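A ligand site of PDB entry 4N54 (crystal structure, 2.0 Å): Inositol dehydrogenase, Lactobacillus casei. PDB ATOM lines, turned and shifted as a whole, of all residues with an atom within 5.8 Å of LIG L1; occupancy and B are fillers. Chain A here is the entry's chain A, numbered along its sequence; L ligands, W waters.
The side-chain carboxylate of Asp 168 lies within hydrogen-bond range of an oxygen (O3) of LIG L1. O6 of LIG L1 lies within hydrogen-bond range of O of Asp 191. The side-chain carboxylate of Asp 191 lies within hydrogen-bond range of an oxygen (O5) of LIG L1, at 2.7 Å. O4 of LIG L1 sits at hydrogen-bond distance from NH2 of Arg 24 (2.7 Å). NE2 of His 195 sits at hydrogen-bond distance from O6 of LIG L1, at 2.7 Å. O6 of LIG L1 is in hydrogen-bond range of NZ of Lys 108 (2.7 Å). OH of Tyr 256 lies within hydrogen-bond range of O2 of LIG L1. O4 of LIG L1 sits at hydrogen-bond distance from NH1 of Arg 250 (3.4 Å). The side-chain carboxylate (OD1) of Asp 191 lies within hydrogen-bond range of an oxygen (O13) of LG2 L2 (3.4 Å). N of Arg 24 sits at hydrogen-bond distance from O2 of LG2 L2 (2.7 Å). An oxygen (O8) of LG2 L2 lies within salt-bridge range of the guanidinium group (NE) of Arg 24, 2.7 Å away. O13 of LG2 L2 lies close to O of Lys 108, at 3.0 Å. NZ of Lys 108 sits close to O13 of LG2 L2 (3.3 Å). SD of Met 137 lies within hydrogen-bond range of N7 of LG2 L2 (3.5 Å).
Water W1 lies within hydrogen-bond range of the guanidinium group of Arg 138 (2.7 Å), the side-chain hydroxyl of Tyr 256 (2.9 Å) and an oxygen (O1) of LIG L1 (3.0 Å).
The guanidinium group (NH1) of Arg 250 is in salt-bridge range of the side-chain carboxylate (OD2) of Asp 168, 2.8 Å away. OD1 of Asp 191 is in salt-bridge range of NZ of Lys 108. The side-chain carboxylate of Asp 191 is in salt-bridge range of the guanidinium group of Arg 250 (2.6 Å). The guanidinium group (NH1) of Arg 250 is in hydrogen-bond range of the side-chain sulfur (SD) of Met 192 (3.5 Å).
Merely in contact with LIG L1: Met 192 (3.5 Å), Phe 296 (3.7 Å) and Phe 179 (3.7 Å). Hydrophobic or aromatic side chains that line LIG L1: Phe 179, Met 192, His 195, Tyr 256 and Phe 296. Of the 14 residues printed, 10 come within 4 Å of LIG L1. The nearest printed residue that does not touch LIG L1 is Met 137 (4.5 Å).
An oxygen (O14) of LG2 L2 is in hydrogen-bond range of an oxygen (O1) of LIG L1 (3.0 Å).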
ATOM      1  N   ARG A  24     -15.146 -25.965  -9.175  1.00  0.00           N
ATOM      2  CA  ARG A  24     -14.899 -24.800  -8.336  1.00  0.00           C
ATOM      3  C   ARG A  24     -13.864 -23.842  -8.895  1.00  0.00           C
ATOM      4  O   ARG A  24     -14.069 -22.650  -8.900  1.00  0.00           O
ATOM      5  CB  ARG A  24     -14.512 -25.230  -6.933  1.00  0.00           C
ATOM      6  CG  ARG A  24     -15.640 -25.846  -6.133  1.00  0.00           C
ATOM      7  CD  ARG A  24     -15.229 -26.190  -4.734  1.00  0.00           C
ATOM      8  NE  ARG A  24     -13.930 -26.828  -4.690  1.00  0.00           N
ATOM      9  CZ  ARG A  24     -13.079 -26.723  -3.688  1.00  0.00           C
ATOM     10  NH1 ARG A  24     -13.373 -25.999  -2.638  1.00  0.00           N
ATOM     11  NH2 ARG A  24     -11.918 -27.332  -3.760  1.00  0.00           N
ATOM     12  N   LYS A 108      -2.296 -27.750  -8.250  1.00  0.00           N
ATOM     13  CA  LYS A 108      -1.770 -28.388  -7.081  1.00  0.00           C
ATOM     14  C   LYS A 108      -2.791 -29.378  -6.548  1.00  0.00           C
ATOM     15  O   LYS A 108      -3.963 -29.271  -6.849  1.00  0.00           O
ATOM     16  CB  LYS A 108      -1.503 -27.323  -6.015  1.00  0.00           C
ATOM     17  CG  LYS A 108      -2.737 -26.493  -5.626  1.00  0.00           C
ATOM     18  CD  LYS A 108      -3.297 -26.926  -4.292  1.00  0.00           C
ATOM     19  CE  LYS A 108      -4.669 -27.516  -4.420  1.00  0.00           C
ATOM     20  NZ  LYS A 108      -5.237 -27.874  -3.127  1.00  0.00           N
ATOM     21  N   MET A 137      -0.285 -20.668  -7.005  1.00  0.00           N
ATOM     22  CA  MET A 137      -0.606 -19.308  -7.360  1.00  0.00           C
ATOM     23  C   MET A 137      -0.172 -18.238  -6.357  1.00  0.00           C
ATOM     24  O   MET A 137      -0.014 -17.094  -6.733  1.00  0.00           O
ATOM     25  CB  MET A 137      -2.094 -19.152  -7.657  1.00  0.00           C
ATOM     26  CG  MET A 137      -2.974 -19.078  -6.435  1.00  0.00           C
ATOM     27  SD  MET A 137      -2.933 -20.533  -5.430  1.00  0.00           S
ATOM     28  CE  MET A 137      -4.065 -20.072  -4.155  1.00  0.00           C
ATOM     29  N   ARG A 138       0.024 -18.603  -5.103  1.00  0.00           N
ATOM     30  CA  ARG A 138       0.470 -17.656  -4.114  1.00  0.00           C
ATOM     31  C   ARG A 138       1.790 -16.987  -4.490  1.00  0.00           C
ATOM     32  O   ARG A 138       2.041 -15.862  -4.130  1.00  0.00           O
ATOM     33  CB  ARG A 138       0.598 -18.308  -2.754  1.00  0.00           C
ATOM     34  CG  ARG A 138      -0.708 -18.587  -2.090  1.00  0.00           C
ATOM     35  CD  ARG A 138      -0.553 -19.095  -0.692  1.00  0.00           C
ATOM     36  NE  ARG A 138      -1.733 -19.831  -0.265  1.00  0.00           N
ATOM     37  CZ  ARG A 138      -1.937 -20.260   0.953  1.00  0.00           C
ATOM     38  NH1 ARG A 138      -1.067 -20.014   1.903  1.00  0.00           N
ATOM     39  NH2 ARG A 138      -3.031 -20.925   1.243  1.00  0.00           N
ATOM     40  N   ASP A 168     -10.471 -22.459   5.137  1.00  0.00           N
ATOM     41  CA  ASP A 168     -11.584 -22.202   4.243  1.00  0.00           C
ATOM     42  C   ASP A 168     -12.761 -21.601   4.995  1.00  0.00           C
ATOM     43  O   ASP A 168     -12.882 -21.780   6.183  1.00  0.00           O
ATOM     44  CB  ASP A 168     -12.018 -23.500   3.546  1.00  0.00           C
ATOM     45  CG  ASP A 168     -11.592 -23.550   2.097  1.00  0.00           C
ATOM     46  OD1 ASP A 168     -11.313 -22.499   1.524  1.00  0.00           O
ATOM     47  OD2 ASP A 168     -11.571 -24.646   1.533  1.00  0.00           O
ATOM     48  N   PHE A 176     -17.575 -27.547  -0.537  1.00  0.00           N
ATOM     49  CA  PHE A 176     -16.461 -28.412  -0.205  1.00  0.00           C
ATOM     50  C   PHE A 176     -16.826 -29.880  -0.184  1.00  0.00           C
ATOM     51  O   PHE A 176     -16.131 -30.697  -0.742  1.00  0.00           O
ATOM     52  CB  PHE A 176     -15.841 -28.052   1.140  1.00  0.00           C
ATOM     53  CG  PHE A 176     -14.765 -28.994   1.567  1.00  0.00           C
ATOM     54  CD1 PHE A 176     -13.632 -29.142   0.814  1.00  0.00           C
ATOM     55  CD2 PHE A 176     -14.895 -29.748   2.695  1.00  0.00           C
ATOM     56  CE1 PHE A 176     -12.667 -30.010   1.187  1.00  0.00           C
ATOM     57  CE2 PHE A 176     -13.930 -30.617   3.068  1.00  0.00           C
ATOM     58  CZ  PHE A 176     -12.811 -30.747   2.314  1.00  0.00           C
ATOM     59  N   PHE A 179     -17.055 -31.342  -3.503  1.00  0.00           N
ATOM     60  CA  PHE A 179     -15.709 -31.516  -3.994  1.00  0.00           C
ATOM     61  C   PHE A 179     -15.024 -32.741  -3.399  1.00  0.00           C
ATOM     62  O   PHE A 179     -14.388 -33.487  -4.115  1.00  0.00           O
ATOM     63  CB  PHE A 179     -14.899 -30.246  -3.702  1.00  0.00           C
ATOM     64  CG  PHE A 179     -13.433 -30.427  -3.795  1.00  0.00           C
ATOM     65  CD1 PHE A 179     -12.810 -30.540  -5.005  1.00  0.00           C
ATOM     66  CD2 PHE A 179     -12.669 -30.446  -2.659  1.00  0.00           C
ATOM     67  CE1 PHE A 179     -11.479 -30.693  -5.072  1.00  0.00           C
ATOM     68  CE2 PHE A 179     -11.329 -30.597  -2.727  1.00  0.00           C
ATOM     69  CZ  PHE A 179     -10.742 -30.727  -3.932  1.00  0.00           C
ATOM     70  N   ASP A 191      -4.389 -31.006   0.280  1.00  0.00           N
ATOM     71  CA  ASP A 191      -5.261 -30.103  -0.449  1.00  0.00           C
ATOM     72  C   ASP A 191      -5.031 -28.642  -0.075  1.00  0.00           C
ATOM     73  O   ASP A 191      -5.057 -27.790  -0.924  1.00  0.00           O
ATOM     74  CB  ASP A 191      -6.726 -30.460  -0.219  1.00  0.00           C
ATOM     75  CG  ASP A 191      -7.647 -29.728  -1.163  1.00  0.00           C
ATOM     76  OD1 ASP A 191      -7.359 -29.681  -2.363  1.00  0.00           O
ATOM     77  OD2 ASP A 191      -8.658 -29.171  -0.689  1.00  0.00           O
ATOM     78  N   MET A 192      -4.815 -28.391   1.211  1.00  0.00           N
ATOM     79  CA  MET A 192      -4.664 -27.040   1.727  1.00  0.00           C
ATOM     80  C   MET A 192      -3.244 -26.722   2.144  1.00  0.00           C
ATOM     81  O   MET A 192      -2.639 -25.792   1.637  1.00  0.00           O
ATOM     82  CB  MET A 192      -5.584 -26.823   2.922  1.00  0.00           C
ATOM     83  CG  MET A 192      -7.027 -26.816   2.592  1.00  0.00           C
ATOM     84  SD  MET A 192      -7.491 -25.487   1.502  1.00  0.00           S
ATOM     85  CE  MET A 192      -7.453 -24.150   2.645  1.00  0.00           C
ATOM     86  N   HIS A 195      -0.025 -25.523  -0.024  1.00  0.00           N
ATOM     87  CA  HIS A 195       0.286 -24.150  -0.382  1.00  0.00           C
ATOM     88  C   HIS A 195       1.295 -23.545   0.588  1.00  0.00           C
ATOM     89  O   HIS A 195       2.209 -22.848   0.185  1.00  0.00           O
ATOM     90  CB  HIS A 195      -0.957 -23.284  -0.341  1.00  0.00           C
ATOM     91  CG  HIS A 195      -1.883 -23.495  -1.494  1.00  0.00           C
ATOM     92  ND1 HIS A 195      -1.652 -22.950  -2.731  1.00  0.00           N
ATOM     93  CD2 HIS A 195      -3.053 -24.163  -1.584  1.00  0.00           C
ATOM     94  CE1 HIS A 195      -2.636 -23.283  -3.540  1.00  0.00           C
ATOM     95  NE2 HIS A 195      -3.507 -24.018  -2.860  1.00  0.00           N
ATOM     96  N   ARG A 250     -11.480 -26.077   7.592  1.00  0.00           N
ATOM     97  CA  ARG A 250     -12.581 -25.890   6.688  1.00  0.00           C
ATOM     98  C   ARG A 250     -13.698 -25.064   7.333  1.00  0.00           C
ATOM     99  O   ARG A 250     -14.725 -24.855   6.724  1.00  0.00           O
ATOM    100  CB  ARG A 250     -13.131 -27.224   6.206  1.00  0.00           C
ATOM    101  CG  ARG A 250     -12.132 -28.138   5.541  1.00  0.00           C
ATOM    102  CD  ARG A 250     -11.647 -27.625   4.220  1.00  0.00           C
ATOM    103  NE  ARG A 250     -10.758 -28.551   3.554  1.00  0.00           N
ATOM    104  CZ  ARG A 250     -10.222 -28.361   2.357  1.00  0.00           C
ATOM    105  NH1 ARG A 250     -10.471 -27.265   1.681  1.00  0.00           N
ATOM    106  NH2 ARG A 250      -9.434 -29.279   1.828  1.00  0.00           N
ATOM    107  N   TYR A 256     -12.380 -16.261   4.431  1.00  0.00           N
ATOM    108  CA  TYR A 256     -11.307 -17.095   3.952  1.00  0.00           C
ATOM    109  C   TYR A 256     -10.043 -16.679   4.649  1.00  0.00           C
ATOM    110  O   TYR A 256      -9.490 -15.640   4.352  1.00  0.00           O
ATOM    111  CB  TYR A 256     -11.175 -16.913   2.450  1.00  0.00           C
ATOM    112  CG  TYR A 256     -10.188 -17.796   1.720  1.00  0.00           C
ATOM    113  CD1 TYR A 256     -10.041 -19.125   2.031  1.00  0.00           C
ATOM    114  CD2 TYR A 256      -9.428 -17.305   0.678  1.00  0.00           C
ATOM    115  CE1 TYR A 256      -9.160 -19.910   1.345  1.00  0.00           C
ATOM    116  CE2 TYR A 256      -8.559 -18.083  -0.008  1.00  0.00           C
ATOM    117  CZ  TYR A 256      -8.426 -19.382   0.320  1.00  0.00           C
ATOM    118  OH  TYR A 256      -7.547 -20.157  -0.367  1.00  0.00           O
ATOM    119  N   PHE A 296     -11.514 -18.359  -2.009  1.00  0.00           N
ATOM    120  CA  PHE A 296     -10.372 -18.308  -2.912  1.00  0.00           C
ATOM    121  C   PHE A 296     -10.550 -17.525  -4.217  1.00  0.00           C
ATOM    122  O   PHE A 296      -9.641 -16.848  -4.607  1.00  0.00           O
ATOM    123  CB  PHE A 296      -9.704 -19.683  -3.135  1.00  0.00           C
ATOM    124  CG  PHE A 296     -10.460 -20.619  -4.035  1.00  0.00           C
ATOM    125  CD1 PHE A 296     -10.288 -20.573  -5.379  1.00  0.00           C
ATOM    126  CD2 PHE A 296     -11.295 -21.573  -3.519  1.00  0.00           C
ATOM    127  CE1 PHE A 296     -10.970 -21.421  -6.184  1.00  0.00           C
ATOM    128  CE2 PHE A 296     -11.968 -22.420  -4.335  1.00  0.00           C
ATOM    129  CZ  PHE A 296     -11.802 -22.333  -5.665  1.00  0.00           C
ATOM    130  N   PHE A 300      -7.673 -14.588  -4.250  1.00  0.00           N
ATOM    131  CA  PHE A 300      -6.570 -14.875  -5.164  1.00  0.00           C
ATOM    132  C   PHE A 300      -6.868 -14.672  -6.631  1.00  0.00           C
ATOM    133  O   PHE A 300      -6.183 -15.211  -7.490  1.00  0.00           O
ATOM    134  CB  PHE A 300      -5.999 -16.273  -4.932  1.00  0.00           C
ATOM    135  CG  PHE A 300      -5.378 -16.457  -3.580  1.00  0.00           C
ATOM    136  CD1 PHE A 300      -4.262 -15.744  -3.220  1.00  0.00           C
ATOM    137  CD2 PHE A 300      -5.902 -17.352  -2.689  1.00  0.00           C
ATOM    138  CE1 PHE A 300      -3.708 -15.907  -1.999  1.00  0.00           C
ATOM    139  CE2 PHE A 300      -5.339 -17.513  -1.469  1.00  0.00           C
ATOM    140  CZ  PHE A 300      -4.236 -16.795  -1.128  1.00  0.00           C
HETATM  141  O1  LIG L   1      -6.931 -22.829  -2.113  1.00  0.00           O
HETATM  142  C1  LIG L   1      -7.576 -23.961  -1.676  1.00  0.00           C
HETATM  143  C2  LIG L   1      -9.063 -23.709  -1.552  1.00  0.00           C
HETATM  144  O2  LIG L   1      -9.290 -22.811  -0.531  1.00  0.00           O
HETATM  145  C3  LIG L   1      -9.777 -24.970  -1.132  1.00  0.00           C
HETATM  146  O3  LIG L   1     -11.115 -24.749  -1.003  1.00  0.00           O
HETATM  147  C4  LIG L   1      -9.522 -26.054  -2.118  1.00  0.00           C
HETATM  148  O4  LIG L   1     -10.172 -27.195  -1.750  1.00  0.00           O
HETATM  149  C5  LIG L   1      -8.080 -26.385  -2.228  1.00  0.00           C
HETATM  150  O5  LIG L   1      -7.933 -27.252  -3.278  1.00  0.00           O
HETATM  151  C6  LIG L   1      -7.211 -25.057  -2.607  1.00  0.00           C
HETATM  152  O6  LIG L   1      -5.872 -25.291  -2.521  1.00  0.00           O
HETATM  153  P1  LG2 L   2     -14.352 -29.732  -8.610  1.00  0.00           P
HETATM  154  O1  LG2 L   2     -14.712 -31.018  -8.059  1.00  0.00           O
HETATM  155  O2  LG2 L   2     -15.063 -28.505  -8.272  1.00  0.00           O
HETATM  156  O3  LG2 L   2     -14.288 -29.804 -10.143  1.00  0.00           O
HETATM  157  C1  LG2 L   2     -13.894 -30.971 -10.793  1.00  0.00           C
HETATM  158  C2  LG2 L   2     -14.026 -30.851 -12.289  1.00  0.00           C
HETATM  159  O4  LG2 L   2     -13.232 -31.875 -12.854  1.00  0.00           O
HETATM  160  C3  LG2 L   2     -15.424 -31.115 -12.796  1.00  0.00           C
HETATM  161  O5  LG2 L   2     -15.589 -30.385 -13.972  1.00  0.00           O
HETATM  162  C4  LG2 L   2     -15.416 -32.554 -13.209  1.00  0.00           C
HETATM  163  O6  LG2 L   2     -16.332 -32.722 -14.278  1.00  0.00           O
HETATM  164  C5  LG2 L   2     -14.004 -32.694 -13.698  1.00  0.00           C
HETATM  165  N1  LG2 L   2     -13.535 -34.074 -13.644  1.00  0.00           N
HETATM  166  C6  LG2 L   2     -13.582 -34.873 -12.596  1.00  0.00           C
HETATM  167  N2  LG2 L   2     -13.066 -36.070 -12.875  1.00  0.00           N
HETATM  168  C7  LG2 L   2     -12.657 -36.047 -14.130  1.00  0.00           C
HETATM  169  C8  LG2 L   2     -12.015 -36.985 -15.062  1.00  0.00           C
HETATM  170  N3  LG2 L   2     -11.717 -38.197 -14.646  1.00  0.00           N
HETATM  171  N4  LG2 L   2     -11.746 -36.587 -16.301  1.00  0.00           N
HETATM  172  C9  LG2 L   2     -12.056 -35.351 -16.679  1.00  0.00           C
HETATM  173  N5  LG2 L   2     -12.634 -34.441 -15.899  1.00  0.00           N
HETATM  174  C10 LG2 L   2     -12.963 -34.724 -14.632  1.00  0.00           C
HETATM  175  O7  LG2 L   2     -12.836 -29.564  -8.230  1.00  0.00           O
HETATM  176  P2  LG2 L   2     -12.092 -28.208  -8.037  1.00  0.00           P
HETATM  177  O8  LG2 L   2     -12.429 -27.676  -6.744  1.00  0.00           O
HETATM  178  O9  LG2 L   2     -12.244 -27.393  -9.216  1.00  0.00           O
HETATM  179  O10 LG2 L   2     -10.607 -28.696  -7.996  1.00  0.00           O
HETATM  180  C11 LG2 L   2      -9.823 -28.874  -9.157  1.00  0.00           C
HETATM  181  C12 LG2 L   2      -8.325 -28.940  -8.893  1.00  0.00           C
HETATM  182  O11 LG2 L   2      -7.846 -27.658  -8.622  1.00  0.00           O
HETATM  183  C13 LG2 L   2      -7.958 -29.815  -7.720  1.00  0.00           C
HETATM  184  O12 LG2 L   2      -6.789 -30.535  -8.029  1.00  0.00           O
HETATM  185  C14 LG2 L   2      -7.687 -28.818  -6.635  1.00  0.00           C
HETATM  186  O13 LG2 L   2      -6.738 -29.269  -5.703  1.00  0.00           O
HETATM  187  C15 LG2 L   2      -7.223 -27.589  -7.388  1.00  0.00           C
HETATM  188  N6  LG2 L   2      -7.655 -26.355  -6.796  1.00  0.00           N
HETATM  189  C16 LG2 L   2      -6.756 -25.439  -6.591  1.00  0.00           C
HETATM  190  C17 LG2 L   2      -7.035 -24.232  -6.046  1.00  0.00           C
HETATM  191  C18 LG2 L   2      -5.932 -23.252  -5.824  1.00  0.00           C
HETATM  192  O14 LG2 L   2      -6.058 -22.440  -4.990  1.00  0.00           O
HETATM  193  N7  LG2 L   2      -4.839 -23.267  -6.523  1.00  0.00           N
HETATM  194  C19 LG2 L   2      -8.452 -23.889  -5.646  1.00  0.00           C
HETATM  195  C20 LG2 L   2      -9.347 -24.981  -5.947  1.00  0.00           C
HETATM  196  C21 LG2 L   2      -8.923 -26.150  -6.497  1.00  0.00           C
HETATM  197  O   HOH W   1      -4.821 -21.078  -0.823  1.00  0.00           O
